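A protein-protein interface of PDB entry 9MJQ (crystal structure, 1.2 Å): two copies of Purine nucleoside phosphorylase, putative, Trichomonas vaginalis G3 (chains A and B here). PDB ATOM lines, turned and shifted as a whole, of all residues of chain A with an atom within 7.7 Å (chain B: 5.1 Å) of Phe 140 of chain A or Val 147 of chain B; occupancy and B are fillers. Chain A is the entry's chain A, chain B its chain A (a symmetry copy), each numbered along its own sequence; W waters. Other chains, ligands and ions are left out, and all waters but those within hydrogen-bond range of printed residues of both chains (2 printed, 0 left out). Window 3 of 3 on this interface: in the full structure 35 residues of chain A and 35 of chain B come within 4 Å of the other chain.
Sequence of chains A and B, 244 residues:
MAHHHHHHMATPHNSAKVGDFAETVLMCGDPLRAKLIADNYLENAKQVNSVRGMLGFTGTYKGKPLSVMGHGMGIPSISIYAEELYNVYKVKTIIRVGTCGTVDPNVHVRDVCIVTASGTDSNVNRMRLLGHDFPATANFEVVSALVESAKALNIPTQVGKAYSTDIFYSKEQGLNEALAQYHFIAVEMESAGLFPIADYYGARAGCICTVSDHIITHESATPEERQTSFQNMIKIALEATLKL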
ATOM      1  N   THR A 116      23.040   3.128 -21.059  1.00  0.00           N
ATOM      2  CA  THR A 116      21.819   2.328 -20.968  1.00  0.00           C
ATOM      3  C   THR A 116      20.547   3.174 -21.045  1.00  0.00           C
ATOM      4  O   THR A 116      19.537   2.715 -21.577  1.00  0.00           O
ATOM      5  CB  THR A 116      21.818   1.554 -19.653  1.00  0.00           C
ATOM      6  OG1 THR A 116      22.053   2.478 -18.587  1.00  0.00           O
ATOM      7  CG2 THR A 116      22.894   0.446 -19.661  1.00  0.00           C
ATOM      8  N   THR A 137      15.700   5.423 -23.272  1.00  0.00           N
ATOM      9  CA  THR A 137      16.297   4.135 -22.960  1.00  0.00           C
ATOM     10  C   THR A 137      16.907   3.548 -24.226  1.00  0.00           C
ATOM     11  O   THR A 137      16.235   3.450 -25.262  1.00  0.00           O
ATOM     12  CB  THR A 137      15.225   3.189 -22.388  1.00  0.00           C
ATOM     13  OG1 THR A 137      14.521   3.831 -21.323  1.00  0.00           O
ATOM     14  CG2 THR A 137      15.862   1.933 -21.857  1.00  0.00           C
ATOM     15  N   ALA A 138      18.162   3.122 -24.131  1.00  0.00           N
ATOM     16  CA  ALA A 138      18.810   2.471 -25.255  1.00  0.00           C
ATOM     17  C   ALA A 138      18.205   1.090 -25.469  1.00  0.00           C
ATOM     18  O   ALA A 138      17.748   0.425 -24.536  1.00  0.00           O
ATOM     19  CB  ALA A 138      20.314   2.341 -25.003  1.00  0.00           C
ATOM     20  N   ASN A 139      18.243   0.643 -26.717  1.00  0.00           N
ATOM     21  CA  ASN A 139      17.804  -0.699 -27.051  1.00  0.00           C
ATOM     22  C   ASN A 139      18.799  -1.717 -26.507  1.00  0.00           C
ATOM     23  O   ASN A 139      20.017  -1.558 -26.642  1.00  0.00           O
ATOM     24  CB  ASN A 139      17.704  -0.817 -28.571  1.00  0.00           C
ATOM     25  CG  ASN A 139      17.473  -2.238 -29.030  1.00  0.00           C
ATOM     26  OD1 ASN A 139      18.415  -2.976 -29.353  1.00  0.00           O
ATOM     27  ND2 ASN A 139      16.217  -2.614 -29.104  1.00  0.00           N
ATOM     28  N   PHE A 140      18.276  -2.785 -25.908  1.00  0.00           N
ATOM     29  CA  PHE A 140      19.145  -3.735 -25.226  1.00  0.00           C
ATOM     30  C   PHE A 140      20.083  -4.450 -26.194  1.00  0.00           C
ATOM     31  O   PHE A 140      21.240  -4.699 -25.855  1.00  0.00           O
ATOM     32  CB  PHE A 140      18.317  -4.746 -24.439  1.00  0.00           C
ATOM     33  CG  PHE A 140      19.144  -5.843 -23.840  1.00  0.00           C
ATOM     34  CD1 PHE A 140      19.890  -5.625 -22.692  1.00  0.00           C
ATOM     35  CD2 PHE A 140      19.241  -7.073 -24.470  1.00  0.00           C
ATOM     36  CE1 PHE A 140      20.680  -6.625 -22.162  1.00  0.00           C
ATOM     37  CE2 PHE A 140      20.024  -8.082 -23.927  1.00  0.00           C
ATOM     38  CZ  PHE A 140      20.753  -7.839 -22.781  1.00  0.00           C
ATOM     39  N   GLU A 141      19.599  -4.826 -27.380  1.00  0.00           N
ATOM     40  CA  GLU A 141      20.472  -5.476 -28.354  1.00  0.00           C
ATOM     41  C   GLU A 141      21.642  -4.573 -28.725  1.00  0.00           C
ATOM     42  O   GLU A 141      22.765  -5.055 -28.914  1.00  0.00           O
ATOM     43  CB  GLU A 141      19.687  -5.875 -29.606  1.00  0.00           C
ATOM     44  CG  GLU A 141      18.676  -7.003 -29.397  1.00  0.00           C
ATOM     45  CD  GLU A 141      18.002  -7.439 -30.690  1.00  0.00           C
ATOM     46  OE1 GLU A 141      17.422  -6.585 -31.394  1.00  0.00           O
ATOM     47  OE2 GLU A 141      18.057  -8.643 -31.008  1.00  0.00           O
ATOM     48  N   VAL A 142      21.394  -3.266 -28.864  1.00  0.00           N
ATOM     49  CA  VAL A 142      22.478  -2.329 -29.170  1.00  0.00           C
ATOM     50  C   VAL A 142      23.459  -2.242 -28.005  1.00  0.00           C
ATOM     51  O   VAL A 142      24.679  -2.317 -28.193  1.00  0.00           O
ATOM     52  CB  VAL A 142      21.925  -0.942 -29.548  1.00  0.00           C
ATOM     53  CG1 VAL A 142      23.070   0.034 -29.789  1.00  0.00           C
ATOM     54  CG2 VAL A 142      21.043  -1.024 -30.780  1.00  0.00           C
ATOM     55  N   VAL A 143      22.944  -2.086 -26.784  1.00  0.00           N
ATOM     56  CA  VAL A 143      23.824  -2.037 -25.621  1.00  0.00           C
ATOM     57  C   VAL A 143      24.679  -3.293 -25.569  1.00  0.00           C
ATOM     58  O   VAL A 143      25.899  -3.232 -25.393  1.00  0.00           O
ATOM     59  CB  VAL A 143      23.013  -1.862 -24.327  1.00  0.00           C
ATOM     60  CG1 VAL A 143      23.938  -1.899 -23.132  1.00  0.00           C
ATOM     61  CG2 VAL A 143      22.213  -0.570 -24.343  1.00  0.00           C
ATOM     62  N   SER A 144      24.039  -4.453 -25.720  1.00  0.00           N
ATOM     63  CA  SER A 144      24.755  -5.719 -25.629  1.00  0.00           C
ATOM     64  C   SER A 144      25.796  -5.840 -26.725  1.00  0.00           C
ATOM     65  O   SER A 144      26.901  -6.337 -26.486  1.00  0.00           O
ATOM     66  CB  SER A 144      23.765  -6.875 -25.743  1.00  0.00           C
ATOM     67  OG  SER A 144      24.425  -8.125 -25.671  1.00  0.00           O
ATOM     68  N   ALA A 145      25.465  -5.402 -27.941  1.00  0.00           N
ATOM     69  CA  ALA A 145      26.439  -5.487 -29.027  1.00  0.00           C
ATOM     70  C   ALA A 145      27.666  -4.645 -28.713  1.00  0.00           C
ATOM     71  O   ALA A 145      28.799  -5.056 -28.985  1.00  0.00           O
ATOM     72  CB  ALA A 145      25.797  -5.074 -30.349  1.00  0.00           C
ATOM     73  N   LEU A 146      27.463  -3.447 -28.164  1.00  0.00           N
ATOM     74  CA  LEU A 146      28.589  -2.609 -27.770  1.00  0.00           C
ATOM     75  C   LEU A 146      29.396  -3.260 -26.654  1.00  0.00           C
ATOM     76  O   LEU A 146      30.630  -3.299 -26.709  1.00  0.00           O
ATOM     77  CB  LEU A 146      28.072  -1.238 -27.342  1.00  0.00           C
ATOM     78  CG  LEU A 146      27.453  -0.402 -28.473  1.00  0.00           C
ATOM     79  CD1 LEU A 146      26.605   0.737 -27.900  1.00  0.00           C
ATOM     80  CD2 LEU A 146      28.523   0.181 -29.374  1.00  0.00           C
ATOM     81  N   VAL A 147      28.720  -3.785 -25.630  1.00  0.00           N
ATOM     82  CA  VAL A 147      29.426  -4.416 -24.513  1.00  0.00           C
ATOM     83  C   VAL A 147      30.256  -5.600 -25.002  1.00  0.00           C
ATOM     84  O   VAL A 147      31.423  -5.763 -24.626  1.00  0.00           O
ATOM     85  CB  VAL A 147      28.424  -4.839 -23.426  1.00  0.00           C
ATOM     86  CG1 VAL A 147      29.074  -5.768 -22.414  1.00  0.00           C
ATOM     87  CG2 VAL A 147      27.850  -3.618 -22.720  1.00  0.00           C
ATOM     88  N   ARG A 204      15.837   1.024 -33.405  1.00  0.00           N
ATOM     89  CA  ARG A 204      16.828   0.799 -32.368  1.00  0.00           C
ATOM     90  C   ARG A 204      17.822   1.940 -32.310  1.00  0.00           C
ATOM     91  O   ARG A 204      18.213   2.492 -33.344  1.00  0.00           O
ATOM     92  CB  ARG A 204      17.591  -0.503 -32.644  1.00  0.00           C
ATOM     93  CG  ARG A 204      16.673  -1.680 -32.572  1.00  0.00           C
ATOM     94  CD  ARG A 204      17.432  -2.935 -32.598  1.00  0.00           C
ATOM     95  NE  ARG A 204      18.236  -3.023 -33.802  1.00  0.00           N
ATOM     96  CZ  ARG A 204      18.865  -4.121 -34.172  1.00  0.00           C
ATOM     97  NH1 ARG A 204      18.790  -5.232 -33.458  1.00  0.00           N
ATOM     98  NH2 ARG A 204      19.585  -4.102 -35.285  1.00  0.00           N
ATOM     99  N   ALA A 205      18.282   2.238 -31.099  1.00  0.00           N
ATOM    100  CA  ALA A 205      19.319   3.230 -30.898  1.00  0.00           C
ATOM    101  C   ALA A 205      20.136   2.891 -29.664  1.00  0.00           C
ATOM    102  O   ALA A 205      19.674   2.212 -28.745  1.00  0.00           O
ATOM    103  CB  ALA A 205      18.742   4.641 -30.762  1.00  0.00           C
ATOM    104  N   LEU A 244      24.279  -6.165 -35.645  1.00  0.00           N
ATOM    105  CA  LEU A 244      23.003  -5.449 -35.634  1.00  0.00           C
ATOM    106  C   LEU A 244      22.391  -5.249 -37.021  1.00  0.00           C
ATOM    107  O   LEU A 244      21.236  -4.820 -37.129  1.00  0.00           O
ATOM    108  CB  LEU A 244      23.205  -4.079 -34.986  1.00  0.00           C
ATOM    109  CG  LEU A 244      23.603  -4.088 -33.506  1.00  0.00           C
ATOM    110  CD1 LEU A 244      24.103  -2.717 -33.112  1.00  0.00           C
ATOM    111  CD2 LEU A 244      22.453  -4.519 -32.602  1.00  0.00           C
ATOM    112  OXT LEU A 244      23.024  -5.485 -38.046  1.00  0.00           O
ATOM    113  N   ILE B 114      11.374  -8.425 -19.474  1.00  0.00           N
ATOM    114  CA  ILE B 114      12.562  -8.030 -18.730  1.00  0.00           C
ATOM    115  C   ILE B 114      12.715  -6.528 -18.928  1.00  0.00           C
ATOM    116  O   ILE B 114      12.795  -6.053 -20.063  1.00  0.00           O
ATOM    117  CB  ILE B 114      13.803  -8.808 -19.198  1.00  0.00           C
ATOM    118  CG1 ILE B 114      13.644 -10.297 -18.857  1.00  0.00           C
ATOM    119  CG2 ILE B 114      15.053  -8.253 -18.548  1.00  0.00           C
ATOM    120  CD1 ILE B 114      14.672 -11.195 -19.495  1.00  0.00           C
ATOM    121  N   THR B 116      14.190  -2.858 -18.928  1.00  0.00           N
ATOM    122  CA  THR B 116      15.440  -2.104 -19.033  1.00  0.00           C
ATOM    123  C   THR B 116      15.383  -0.757 -18.311  1.00  0.00           C
ATOM    124  O   THR B 116      16.397  -0.304 -17.781  1.00  0.00           O
ATOM    125  CB  THR B 116      15.762  -1.862 -20.505  1.00  0.00           C
ATOM    126  OG1 THR B 116      14.614  -1.279 -21.127  1.00  0.00           O
ATOM    127  CG2 THR B 116      16.154  -3.179 -21.210  1.00  0.00           C
ATOM    128  N   PHE B 140      22.667  -3.077 -15.884  1.00  0.00           N
ATOM    129  CA  PHE B 140      22.861  -3.882 -17.083  1.00  0.00           C
ATOM    130  C   PHE B 140      23.229  -5.325 -16.750  1.00  0.00           C
ATOM    131  O   PHE B 140      22.781  -6.246 -17.433  1.00  0.00           O
ATOM    132  CB  PHE B 140      23.921  -3.254 -17.983  1.00  0.00           C
ATOM    133  CG  PHE B 140      24.278  -4.113 -19.158  1.00  0.00           C
ATOM    134  CD1 PHE B 140      23.445  -4.187 -20.264  1.00  0.00           C
ATOM    135  CD2 PHE B 140      25.409  -4.912 -19.125  1.00  0.00           C
ATOM    136  CE1 PHE B 140      23.757  -5.007 -21.329  1.00  0.00           C
ATOM    137  CE2 PHE B 140      25.729  -5.723 -20.204  1.00  0.00           C
ATOM    138  CZ  PHE B 140      24.884  -5.776 -21.294  1.00  0.00           C
ATOM    139  N   VAL B 142      22.248  -7.054 -14.241  1.00  0.00           N
ATOM    140  CA  VAL B 142      21.006  -7.728 -13.858  1.00  0.00           C
ATOM    141  C   VAL B 142      20.161  -8.041 -15.089  1.00  0.00           C
ATOM    142  O   VAL B 142      19.665  -9.163 -15.253  1.00  0.00           O
ATOM    143  CB  VAL B 142      20.216  -6.899 -12.827  1.00  0.00           C
ATOM    144  CG1 VAL B 142      18.894  -7.584 -12.501  1.00  0.00           C
ATOM    145  CG2 VAL B 142      21.024  -6.694 -11.559  1.00  0.00           C
ATOM    146  N   VAL B 143      19.987  -7.059 -15.975  1.00  0.00           N
ATOM    147  CA  VAL B 143      19.224  -7.302 -17.195  1.00  0.00           C
ATOM    148  C   VAL B 143      19.835  -8.466 -17.960  1.00  0.00           C
ATOM    149  O   VAL B 143      19.137  -9.388 -18.389  1.00  0.00           O
ATOM    150  CB  VAL B 143      19.164  -6.037 -18.065  1.00  0.00           C
ATOM    151  CG1 VAL B 143      18.442  -6.337 -19.359  1.00  0.00           C
ATOM    152  CG2 VAL B 143      18.486  -4.891 -17.331  1.00  0.00           C
ATOM    153  N   SER B 144      21.156  -8.431 -18.140  1.00  0.00           N
ATOM    154  CA  SER B 144      21.834  -9.466 -18.909  1.00  0.00           C
ATOM    155  C   SER B 144      21.687 -10.824 -18.247  1.00  0.00           C
ATOM    156  O   SER B 144      21.496 -11.834 -18.931  1.00  0.00           O
ATOM    157  CB  SER B 144      23.315  -9.122 -19.033  1.00  0.00           C
ATOM    158  OG  SER B 144      24.011 -10.114 -19.765  1.00  0.00           O
ATOM    159  N   ALA B 145      21.785 -10.875 -16.918  1.00  0.00           N
ATOM    160  CA  ALA B 145      21.639 -12.159 -16.235  1.00  0.00           C
ATOM    161  C   ALA B 145      20.252 -12.737 -16.471  1.00  0.00           C
ATOM    162  O   ALA B 145      20.101 -13.947 -16.676  1.00  0.00           O
ATOM    163  CB  ALA B 145      21.937 -12.005 -14.745  1.00  0.00           C
ATOM    164  N   LEU B 146      19.220 -11.895 -16.420  1.00  0.00           N
ATOM    165  CA  LEU B 146      17.868 -12.359 -16.703  1.00  0.00           C
ATOM    166  C   LEU B 146      17.736 -12.825 -18.148  1.00  0.00           C
ATOM    167  O   LEU B 146      17.171 -13.889 -18.418  1.00  0.00           O
ATOM    168  CB  LEU B 146      16.876 -11.239 -16.397  1.00  0.00           C
ATOM    169  CG  LEU B 146      16.763 -10.867 -14.911  1.00  0.00           C
ATOM    170  CD1 LEU B 146      16.094  -9.500 -14.747  1.00  0.00           C
ATOM    171  CD2 LEU B 146      15.969 -11.904 -14.144  1.00  0.00           C
ATOM    172  N   VAL B 147      18.257 -12.043 -19.097  1.00  0.00           N
ATOM    173  CA  VAL B 147      18.159 -12.417 -20.509  1.00  0.00           C
ATOM    174  C   VAL B 147      18.855 -13.752 -20.762  1.00  0.00           C
ATOM    175  O   VAL B 147      18.320 -14.633 -21.445  1.00  0.00           O
ATOM    176  CB  VAL B 147      18.742 -11.300 -21.392  1.00  0.00           C
ATOM    177  CG1 VAL B 147      18.945 -11.782 -22.819  1.00  0.00           C
ATOM    178  CG2 VAL B 147      17.836 -10.076 -21.379  1.00  0.00           C
ATOM    179  N   GLU B 148      20.062 -13.914 -20.224  1.00  0.00           N
ATOM    180  CA  GLU B 148      20.830 -15.123 -20.486  1.00  0.00           C
ATOM    181  C   GLU B 148      20.217 -16.328 -19.802  1.00  0.00           C
ATOM    182  O   GLU B 148      20.262 -17.437 -20.334  1.00  0.00           O
ATOM    183  CB  GLU B 148      22.268 -14.924 -20.025  1.00  0.00           C
ATOM    184  CG  GLU B 148      23.033 -13.946 -20.887  1.00  0.00           C
ATOM    185  CD  GLU B 148      22.980 -14.316 -22.368  1.00  0.00           C
ATOM    186  OE1 GLU B 148      23.352 -15.462 -22.695  1.00  0.00           O
ATOM    187  OE2 GLU B 148      22.524 -13.477 -23.183  1.00  0.00           O
ATOM    188  N   SER B 149      19.659 -16.137 -18.610  1.00  0.00           N
ATOM    189  CA  SER B 149      18.983 -17.237 -17.933  1.00  0.00           C
ATOM    190  C   SER B 149      17.768 -17.703 -18.725  1.00  0.00           C
ATOM    191  O   SER B 149      17.559 -18.907 -18.897  1.00  0.00           O
ATOM    192  CB  SER B 149      18.591 -16.836 -16.509  1.00  0.00           C
ATOM    193  OG  SER B 149      19.739 -16.562 -15.715  1.00  0.00           O
ATOM    194  N   ALA B 150      16.958 -16.764 -19.230  1.00  0.00           N
ATOM    195  CA  ALA B 150      15.812 -17.145 -20.050  1.00  0.00           C
ATOM    196  C   ALA B 150      16.248 -17.899 -21.297  1.00  0.00           C
ATOM    197  O   ALA B 150      15.616 -18.889 -21.683  1.00  0.00           O
ATOM    198  CB  ALA B 150      15.007 -15.905 -20.436  1.00  0.00           C
ATOM    199  N   LYS B 151      17.326 -17.449 -21.939  1.00  0.00           N
ATOM    200  CA  LYS B 151      17.847 -18.161 -23.106  1.00  0.00           C
ATOM    201  C   LYS B 151      18.227 -19.594 -22.759  1.00  0.00           C
ATOM    202  O   LYS B 151      17.903 -20.532 -23.498  1.00  0.00           O
ATOM    203  CB  LYS B 151      19.069 -17.429 -23.654  1.00  0.00           C
ATOM    204  CG  LYS B 151      18.763 -16.148 -24.395  1.00  0.00           C
ATOM    205  CD  LYS B 151      20.056 -15.494 -24.844  1.00  0.00           C
ATOM    206  CE  LYS B 151      19.823 -14.233 -25.636  1.00  0.00           C
ATOM    207  NZ  LYS B 151      21.120 -13.548 -25.891  1.00  0.00           N
ATOM    208  N   VAL B 159      12.011  -7.572 -24.046  1.00  0.00           N
ATOM    209  CA  VAL B 159      12.988  -6.782 -23.306  1.00  0.00           C
ATOM    210  C   VAL B 159      12.736  -5.319 -23.649  1.00  0.00           C
ATOM    211  O   VAL B 159      12.787  -4.934 -24.825  1.00  0.00           O
ATOM    212  CB  VAL B 159      14.425  -7.189 -23.676  1.00  0.00           C
ATOM    213  CG1 VAL B 159      15.442  -6.394 -22.880  1.00  0.00           C
ATOM    214  CG2 VAL B 159      14.633  -8.673 -23.438  1.00  0.00           C
HETATM  215  O   HOH W   1      15.486  -3.078 -25.486  1.00  0.00           O
HETATM  216  O   HOH W   2      15.374  -1.016 -23.774  1.00  0.00           O
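Among the printed residues, merely in contact across the chains: Thr 137 of chain A with Thr 116 of chain B, Phe 140 of chain A with Phe 140 of chain B, Val 143 of chain A with Phe 140 of chain B, Phe 140 of chain A with Val 143 of chain B, Phe 140 of chain A with Val 159 of chain B, Phe 140 of chain A with Val 147 of chain B and Val 147 of chain A with Phe 140 of chain B.
Water W2 bridges the side-chain hydroxyl (OG1) of Thr 116 of chain B (2.8 Å) and the backbone carbonyl oxygen (O) of Ala 138 of chain A (2.9 Å). Water W1 lies within hydrogen-bond range of N of Phe 140 of chain A (2.8 Å) and O of Val 159 of chain B (3.3 Å).
Phe 140 of chain A touches its own counterpart, Phe 140 of chain B. Phe 140 of chain A touches Val 143 of chain B, and with the chains exchanged Val 143 of chain A touches Phe 140 of chain B. Phe 140 of chain A touches Val 147 of chain B, and with the chains exchanged Val 147 of chain A touches Phe 140 of chain B. Positions printed for both chains: 116, 140, 142, 143, 144, 145, 146 and 147.
Phe 140 of chain A touches just these residues of chain B: Phe 140, Val 143, Val 147 and Val 159. Of the printed residues of chain B, Val 147 of chain A touches Phe 140. Of the printed residues of chain A, Phe 140 of chain B touches Phe 140 (3.6 Å), Val 143 (3.6 Å) and Val 147 (3.9 Å). Printed residues of chain A within 4 Å of Val 143 of chain B: Phe 140 (3.6 Å). Ser 144 of chain B touches none of the printed residues of chain A. Val 147 of chain B touches just one residue of chain A: Phe 140. Of the printed residues of chain A, Val 159 of chain B touches Phe 140. The nearest residue of chain B that does not touch Phe 140 of chain A is Thr 116 of chain B (4.2 Å).
Printed residues of chain A that touch a printed residue of chain B: Thr 137, Phe 140, Val 143 and Val 147. Of the 14 printed residues of chain B, 5 touch a printed residue of chain A. Printed residues of chain B that touch a printed residue of chain A: Thr 116, Phe 140, Val 143, Val 147 and Val 159. Among the printed residues, 7 pairs touch across the chains. Among the printed residues, no Asp or Glu carboxylate lies within 4 Å of a Lys or Arg side-chain nitrogen of the other chain.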
